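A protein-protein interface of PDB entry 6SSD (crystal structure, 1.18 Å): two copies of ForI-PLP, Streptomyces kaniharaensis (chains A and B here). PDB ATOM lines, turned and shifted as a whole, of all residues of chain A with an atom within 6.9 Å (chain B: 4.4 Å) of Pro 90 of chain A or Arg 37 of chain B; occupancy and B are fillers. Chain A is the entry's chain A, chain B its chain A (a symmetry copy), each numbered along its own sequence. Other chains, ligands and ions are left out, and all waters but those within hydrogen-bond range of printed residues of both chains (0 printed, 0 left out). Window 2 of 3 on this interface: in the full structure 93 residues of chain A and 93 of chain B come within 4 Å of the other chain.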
ATOM      1  N   HIS A  81      -0.551  24.653  -1.145  1.00  0.00           N
ATOM      2  CA  HIS A  81      -0.009  25.638  -0.203  1.00  0.00           C
ATOM      3  C   HIS A  81       0.898  25.032   0.880  1.00  0.00           C
ATOM      4  O   HIS A  81       1.492  25.793   1.619  1.00  0.00           O
ATOM      5  CB  HIS A  81      -1.138  26.421   0.453  1.00  0.00           C
ATOM      6  CG  HIS A  81      -1.792  27.391  -0.464  1.00  0.00           C
ATOM      7  ND1 HIS A  81      -3.134  27.385  -0.758  1.00  0.00           N
ATOM      8  CD2 HIS A  81      -1.264  28.456  -1.104  1.00  0.00           C
ATOM      9  CE1 HIS A  81      -3.400  28.382  -1.590  1.00  0.00           C
ATOM     10  NE2 HIS A  81      -2.285  29.041  -1.819  1.00  0.00           N
ATOM     11  N   GLY A  82       0.990  23.702   0.934  1.00  0.00           N
ATOM     12  CA  GLY A  82       1.813  23.022   1.924  1.00  0.00           C
ATOM     13  C   GLY A  82       0.998  22.013   2.727  1.00  0.00           C
ATOM     14  O   GLY A  82      -0.062  22.330   3.239  1.00  0.00           O
ATOM     15  N   PHE A  85       2.806  21.722   8.577  1.00  0.00           N
ATOM     16  CA  PHE A  85       3.669  22.779   9.076  1.00  0.00           C
ATOM     17  C   PHE A  85       3.912  22.553  10.560  1.00  0.00           C
ATOM     18  O   PHE A  85       3.072  22.019  11.258  1.00  0.00           O
ATOM     19  CB  PHE A  85       3.003  24.158   8.943  1.00  0.00           C
ATOM     20  CG  PHE A  85       2.744  24.602   7.527  1.00  0.00           C
ATOM     21  CD1 PHE A  85       3.701  25.304   6.810  1.00  0.00           C
ATOM     22  CD2 PHE A  85       1.544  24.329   6.905  1.00  0.00           C
ATOM     23  CE1 PHE A  85       3.468  25.743   5.526  1.00  0.00           C
ATOM     24  CE2 PHE A  85       1.310  24.746   5.599  1.00  0.00           C
ATOM     25  CZ  PHE A  85       2.277  25.442   4.927  1.00  0.00           C
ATOM     26  N   PRO A  88       0.704  26.590  13.643  1.00  0.00           N
ATOM     27  CA  PRO A  88      -0.710  26.513  13.349  1.00  0.00           C
ATOM     28  C   PRO A  88      -1.076  27.368  12.130  1.00  0.00           C
ATOM     29  O   PRO A  88      -0.288  28.231  11.727  1.00  0.00           O
ATOM     30  CB  PRO A  88      -1.374  26.984  14.647  1.00  0.00           C
ATOM     31  CG  PRO A  88      -0.392  27.953  15.227  1.00  0.00           C
ATOM     32  CD  PRO A  88       0.979  27.362  14.877  1.00  0.00           C
ATOM     33  N   THR A  89      -2.270  27.138  11.591  1.00  0.00           N
ATOM     34  CA  THR A  89      -2.728  27.750  10.342  1.00  0.00           C
ATOM     35  C   THR A  89      -4.127  28.326  10.506  1.00  0.00           C
ATOM     36  O   THR A  89      -4.876  27.918  11.397  1.00  0.00           O
ATOM     37  CB  THR A  89      -2.760  26.720   9.190  1.00  0.00           C
ATOM     38  OG1 THR A  89      -3.769  25.723   9.463  1.00  0.00           O
ATOM     39  CG2 THR A  89      -1.400  26.101   8.923  1.00  0.00           C
ATOM     40  N   PRO A  90      -4.553  29.222   9.600  1.00  0.00           N
ATOM     41  CA  PRO A  90      -5.925  29.720   9.682  1.00  0.00           C
ATOM     42  C   PRO A  90      -6.985  28.624   9.608  1.00  0.00           C
ATOM     43  O   PRO A  90      -8.008  28.730  10.291  1.00  0.00           O
ATOM     44  CB  PRO A  90      -6.037  30.664   8.474  1.00  0.00           C
ATOM     45  CG  PRO A  90      -4.648  31.123   8.245  1.00  0.00           C
ATOM     46  CD  PRO A  90      -3.753  29.974   8.618  1.00  0.00           C
ATOM     47  N   VAL A  91      -6.774  27.596   8.793  1.00  0.00           N
ATOM     48  CA  VAL A  91      -7.828  26.617   8.600  1.00  0.00           C
ATOM     49  C   VAL A  91      -8.088  25.775   9.858  1.00  0.00           C
ATOM     50  O   VAL A  91      -9.211  25.284  10.033  1.00  0.00           O
ATOM     51  CB  VAL A  91      -7.662  25.711   7.361  1.00  0.00           C
ATOM     52  CG1 VAL A  91      -7.971  26.480   6.085  1.00  0.00           C
ATOM     53  CG2 VAL A  91      -6.332  24.982   7.347  1.00  0.00           C
ATOM     54  N   GLU A  92      -7.109  25.585  10.757  1.00  0.00           N
ATOM     55  CA  GLU A  92      -7.424  24.863  11.981  1.00  0.00           C
ATOM     56  C   GLU A  92      -8.431  25.623  12.814  1.00  0.00           C
ATOM     57  O   GLU A  92      -9.266  25.019  13.487  1.00  0.00           O
ATOM     58  CB  GLU A  92      -6.192  24.477  12.800  1.00  0.00           C
ATOM     59  CG  GLU A  92      -5.536  25.569  13.620  1.00  0.00           C
ATOM     60  CD  GLU A  92      -4.370  25.075  14.452  1.00  0.00           C
ATOM     61  OE1 GLU A  92      -3.428  24.507  13.868  1.00  0.00           O
ATOM     62  OE2 GLU A  92      -4.383  25.274  15.687  1.00  0.00           O
ATOM     63  N   VAL A  93      -8.330  26.950  12.837  1.00  0.00           N
ATOM     64  CA  VAL A  93      -9.272  27.768  13.593  1.00  0.00           C
ATOM     65  C   VAL A  93     -10.660  27.738  12.954  1.00  0.00           C
ATOM     66  O   VAL A  93     -11.680  27.572  13.631  1.00  0.00           O
ATOM     67  CB  VAL A  93      -8.715  29.202  13.774  1.00  0.00           C
ATOM     68  CG1 VAL A  93      -9.637  30.003  14.672  1.00  0.00           C
ATOM     69  CG2 VAL A  93      -7.291  29.181  14.328  1.00  0.00           C
ATOM     70  N   GLU A  94     -10.703  27.891  11.633  1.00  0.00           N
ATOM     71  CA  GLU A  94     -11.955  27.828  10.910  1.00  0.00           C
ATOM     72  C   GLU A  94     -12.669  26.487  11.144  1.00  0.00           C
ATOM     73  O   GLU A  94     -13.884  26.463  11.384  1.00  0.00           O
ATOM     74  CB  GLU A  94     -11.708  28.072   9.419  1.00  0.00           C
ATOM     75  CG  GLU A  94     -12.977  28.046   8.578  1.00  0.00           C
ATOM     76  CD  GLU A  94     -12.786  28.274   7.097  1.00  0.00           C
ATOM     77  OE1 GLU A  94     -11.734  28.734   6.688  1.00  0.00           O
ATOM     78  OE2 GLU A  94     -13.721  27.957   6.323  1.00  0.00           O
ATOM     79  N   TYR A  95     -11.903  25.394  11.046  1.00  0.00           N
ATOM     80  CA  TYR A  95     -12.494  24.077  11.222  1.00  0.00           C
ATOM     81  C   TYR A  95     -12.910  23.808  12.662  1.00  0.00           C
ATOM     82  O   TYR A  95     -13.978  23.244  12.900  1.00  0.00           O
ATOM     83  CB  TYR A  95     -11.570  22.974  10.707  1.00  0.00           C
ATOM     84  CG  TYR A  95     -12.201  21.588  10.730  1.00  0.00           C
ATOM     85  CD1 TYR A  95     -13.403  21.313  10.116  1.00  0.00           C
ATOM     86  CD2 TYR A  95     -11.573  20.561  11.417  1.00  0.00           C
ATOM     87  CE1 TYR A  95     -13.965  20.044  10.154  1.00  0.00           C
ATOM     88  CE2 TYR A  95     -12.124  19.309  11.440  1.00  0.00           C
ATOM     89  CZ  TYR A  95     -13.309  19.061  10.829  1.00  0.00           C
ATOM     90  OH  TYR A  95     -13.828  17.772  10.862  1.00  0.00           O
ATOM     91  N   PRO A 303      -3.276  21.329   7.491  1.00  0.00           N
ATOM     92  CA  PRO A 303      -4.264  22.083   6.727  1.00  0.00           C
ATOM     93  C   PRO A 303      -4.962  21.264   5.650  1.00  0.00           C
ATOM     94  O   PRO A 303      -6.046  21.672   5.183  1.00  0.00           O
ATOM     95  CB  PRO A 303      -3.431  23.229   6.128  1.00  0.00           C
ATOM     96  CG  PRO A 303      -2.009  22.744   6.179  1.00  0.00           C
ATOM     97  CD  PRO A 303      -1.931  21.930   7.421  1.00  0.00           C
ATOM     98  N   MET A 306      -7.726  19.639   7.659  1.00  0.00           N
ATOM     99  CA  MET A 306      -8.652  20.702   8.052  1.00  0.00           C
ATOM    100  C   MET A 306      -9.501  21.148   6.869  1.00  0.00           C
ATOM    101  O   MET A 306     -10.704  21.392   7.031  1.00  0.00           O
ATOM    102  CB  MET A 306      -7.927  21.909   8.629  1.00  0.00           C
ATOM    103  CG  MET A 306      -7.089  21.676   9.869  1.00  0.00           C
ATOM    104  SD  MET A 306      -7.909  21.192  11.379  1.00  0.00           S
ATOM    105  CE  MET A 306      -8.069  19.394  11.172  1.00  0.00           C
ATOM    106  N   ILE A 310     -13.495  21.132   6.576  1.00  0.00           N
ATOM    107  CA  ILE A 310     -14.346  22.299   6.282  1.00  0.00           C
ATOM    108  C   ILE A 310     -15.289  21.975   5.141  1.00  0.00           C
ATOM    109  O   ILE A 310     -16.478  22.325   5.200  1.00  0.00           O
ATOM    110  CB  ILE A 310     -13.431  23.504   5.937  1.00  0.00           C
ATOM    111  CG1 ILE A 310     -12.717  24.019   7.201  1.00  0.00           C
ATOM    112  CG2 ILE A 310     -14.226  24.597   5.220  1.00  0.00           C
ATOM    113  CD1 ILE A 310     -11.501  24.887   6.992  1.00  0.00           C
ATOM    114  N   LYS B   6      -2.085  39.526  12.713  1.00  0.00           N
ATOM    115  CA  LYS B   6      -2.995  38.536  12.149  1.00  0.00           C
ATOM    116  C   LYS B   6      -2.875  37.211  12.936  1.00  0.00           C
ATOM    117  O   LYS B   6      -3.886  36.511  13.128  1.00  0.00           O
ATOM    118  CB  LYS B   6      -2.805  38.380  10.636  1.00  0.00           C
ATOM    119  CG  LYS B   6      -3.327  39.636   9.863  1.00  0.00           C
ATOM    120  CD  LYS B   6      -3.185  39.563   8.363  1.00  0.00           C
ATOM    121  CE  LYS B   6      -3.571  40.882   7.701  1.00  0.00           C
ATOM    122  NZ  LYS B   6      -3.221  40.860   6.279  1.00  0.00           N
ATOM    123  N   LEU B  10      -6.015  35.365  15.024  1.00  0.00           N
ATOM    124  CA  LEU B  10      -6.317  33.935  14.921  1.00  0.00           C
ATOM    125  C   LEU B  10      -6.311  33.297  16.312  1.00  0.00           C
ATOM    126  O   LEU B  10      -7.205  32.504  16.642  1.00  0.00           O
ATOM    127  CB  LEU B  10      -5.323  33.221  14.002  1.00  0.00           C
ATOM    128  CG  LEU B  10      -5.600  33.452  12.527  1.00  0.00           C
ATOM    129  CD1 LEU B  10      -4.385  33.103  11.665  1.00  0.00           C
ATOM    130  CD2 LEU B  10      -6.825  32.693  12.062  1.00  0.00           C
ATOM    131  N   VAL B  36       0.945  30.378  10.239  1.00  0.00           N
ATOM    132  CA  VAL B  36       1.446  30.435   8.871  1.00  0.00           C
ATOM    133  C   VAL B  36       0.348  30.144   7.854  1.00  0.00           C
ATOM    134  O   VAL B  36      -0.643  29.476   8.169  1.00  0.00           O
ATOM    135  CB  VAL B  36       2.652  29.521   8.667  1.00  0.00           C
ATOM    136  CG1 VAL B  36       3.764  29.882   9.635  1.00  0.00           C
ATOM    137  CG2 VAL B  36       2.287  28.050   8.738  1.00  0.00           C
ATOM    138  N   ARG B  37       0.542  30.684   6.646  1.00  0.00           N
ATOM    139  CA  ARG B  37      -0.452  30.581   5.596  1.00  0.00           C
ATOM    140  C   ARG B  37      -0.049  29.604   4.481  1.00  0.00           C
ATOM    141  O   ARG B  37      -0.893  28.884   3.960  1.00  0.00           O
ATOM    142  CB  ARG B  37      -0.747  31.977   4.984  1.00  0.00           C
ATOM    143  CG  ARG B  37      -2.014  32.031   4.161  1.00  0.00           C
ATOM    144  CD  ARG B  37      -2.359  33.446   3.728  1.00  0.00           C
ATOM    145  NE  ARG B  37      -2.484  34.468   4.792  1.00  0.00           N
ATOM    146  CZ  ARG B  37      -3.558  34.691   5.563  1.00  0.00           C
ATOM    147  NH1 ARG B  37      -4.643  33.948   5.434  1.00  0.00           N
ATOM    148  NH2 ARG B  37      -3.564  35.699   6.475  1.00  0.00           N
ATOM    149  N   SER B  38       1.210  29.608   4.072  1.00  0.00           N
ATOM    150  CA  SER B  38       1.652  28.773   2.952  1.00  0.00           C
ATOM    151  C   SER B  38       3.152  28.608   2.999  1.00  0.00           C
ATOM    152  O   SER B  38       3.861  29.354   3.696  1.00  0.00           O
ATOM    153  CB  SER B  38       1.261  29.417   1.629  1.00  0.00           C
ATOM    154  OG  SER B  38       1.958  30.646   1.450  1.00  0.00           O
ATOM    155  N   THR B  45       5.557  31.468   4.514  1.00  0.00           N
ATOM    156  CA  THR B  45       4.991  32.807   4.661  1.00  0.00           C
ATOM    157  C   THR B  45       3.967  32.780   5.788  1.00  0.00           C
ATOM    158  O   THR B  45       2.988  32.001   5.749  1.00  0.00           O
ATOM    159  CB  THR B  45       4.375  33.266   3.335  1.00  0.00           C
ATOM    160  OG1 THR B  45       5.391  33.274   2.338  1.00  0.00           O
ATOM    161  CG2 THR B  45       3.756  34.648   3.455  1.00  0.00           C
ATOM    162  N   ASP B  46       4.169  33.645   6.781  1.00  0.00           N
ATOM    163  CA  ASP B  46       3.261  33.705   7.902  1.00  0.00           C
ATOM    164  C   ASP B  46       1.996  34.458   7.534  1.00  0.00           C
ATOM    165  O   ASP B  46       1.869  35.014   6.444  1.00  0.00           O
ATOM    166  CB  ASP B  46       3.968  34.189   9.180  1.00  0.00           C
ATOM    167  CG  ASP B  46       4.122  35.697   9.324  1.00  0.00           C
ATOM    168  OD1 ASP B  46       3.632  36.461   8.461  1.00  0.00           O
ATOM    169  OD2 ASP B  46       4.776  36.072  10.335  1.00  0.00           O
ATOM    170  N   VAL B  47       1.018  34.430   8.443  1.00  0.00           N
ATOM    171  CA  VAL B  47      -0.276  35.041   8.164  1.00  0.00           C
ATOM    172  C   VAL B  47      -0.198  36.572   8.054  1.00  0.00           C
ATOM    173  O   VAL B  47      -1.119  37.181   7.488  1.00  0.00           O
ATOM    174  CB  VAL B  47      -1.354  34.637   9.170  1.00  0.00           C
ATOM    175  CG1 VAL B  47      -1.651  33.138   9.022  1.00  0.00           C
ATOM    176  CG2 VAL B  47      -0.976  35.014  10.587  1.00  0.00           C
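No position is printed for both chains.
Of the 9 pairs that touch across the chains among the printed residues, none has its exchanged pair printed and touching as well.
Among the printed residues, pairs that only touch across the chains: Pro 90 of chain A with Val 36 of chain B, His 81 of chain A with Ser 38 of chain B, Thr 89 of chain A with Val 36 of chain B, Phe 85 of chain A with Val 36 of chain B, Pro 90 of chain A with Val 47 of chain B, Phe 85 of chain A with Ser 38 of chain B, Pro 90 of chain A with Leu 10 of chain B and Pro 90 of chain A with Arg 37 of chain B.
The backbone carbonyl oxygen (O) of Pro 88 of chain A lies within hydrogen-bond range of the backbone NH (N) of Val 36 of chain B.
Hydrophobic or aromatic side chains of chain A within 4 Å of the printed part of chain B: His 81, Phe 85 and Pro 90.
Of the printed residues of chain B, Pro 90 of chain A touches Leu 10 (3.9 Å), Val 36 (3.2 Å), Arg 37 (3.99 Å) and Val 47 (3.7 Å).
Printed residues of chain A within 4 Å of Arg 37 of chain B: Pro 90.
Of the printed residues of chain A, Leu 10 of chain B touches Pro 90.
Of the printed residues of chain A, Val 47 of chain B touches Pro 90.
Printed residues of chain A within 4 Å of Val 36 of chain B: Phe 85, Pro 88, Thr 89 and Pro 90.
Of the printed residues of chain B, Thr 89 of chain A touches Val 36 (3.5 Å).
Of the printed residues of chain B, Phe 85 of chain A touches Val 36 and Ser 38.
Val 93 of chain A touches none of the printed residues of chain B.
Glu 94 of chain A touches none of the printed residues of chain B.
The nearest printed residue of chain B that does not touch Phe 85 of chain A is Arg 37 of chain B (4.8 Å).
The backbone carbonyl oxygen (O) of Thr 45 of chain B lies within hydrogen-bond range of the backbone NH (N) of Arg 37 of chain B (2.9 Å).
The backbone carbonyl oxygen of Val 47 of chain B is in hydrogen-bond range of the guanidinium group of Arg 37 of chain B, 3.0 Å away.
N of Thr 45 of chain B sits at hydrogen-bond distance from O of Ser 38 of chain B, 2.8 Å away.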
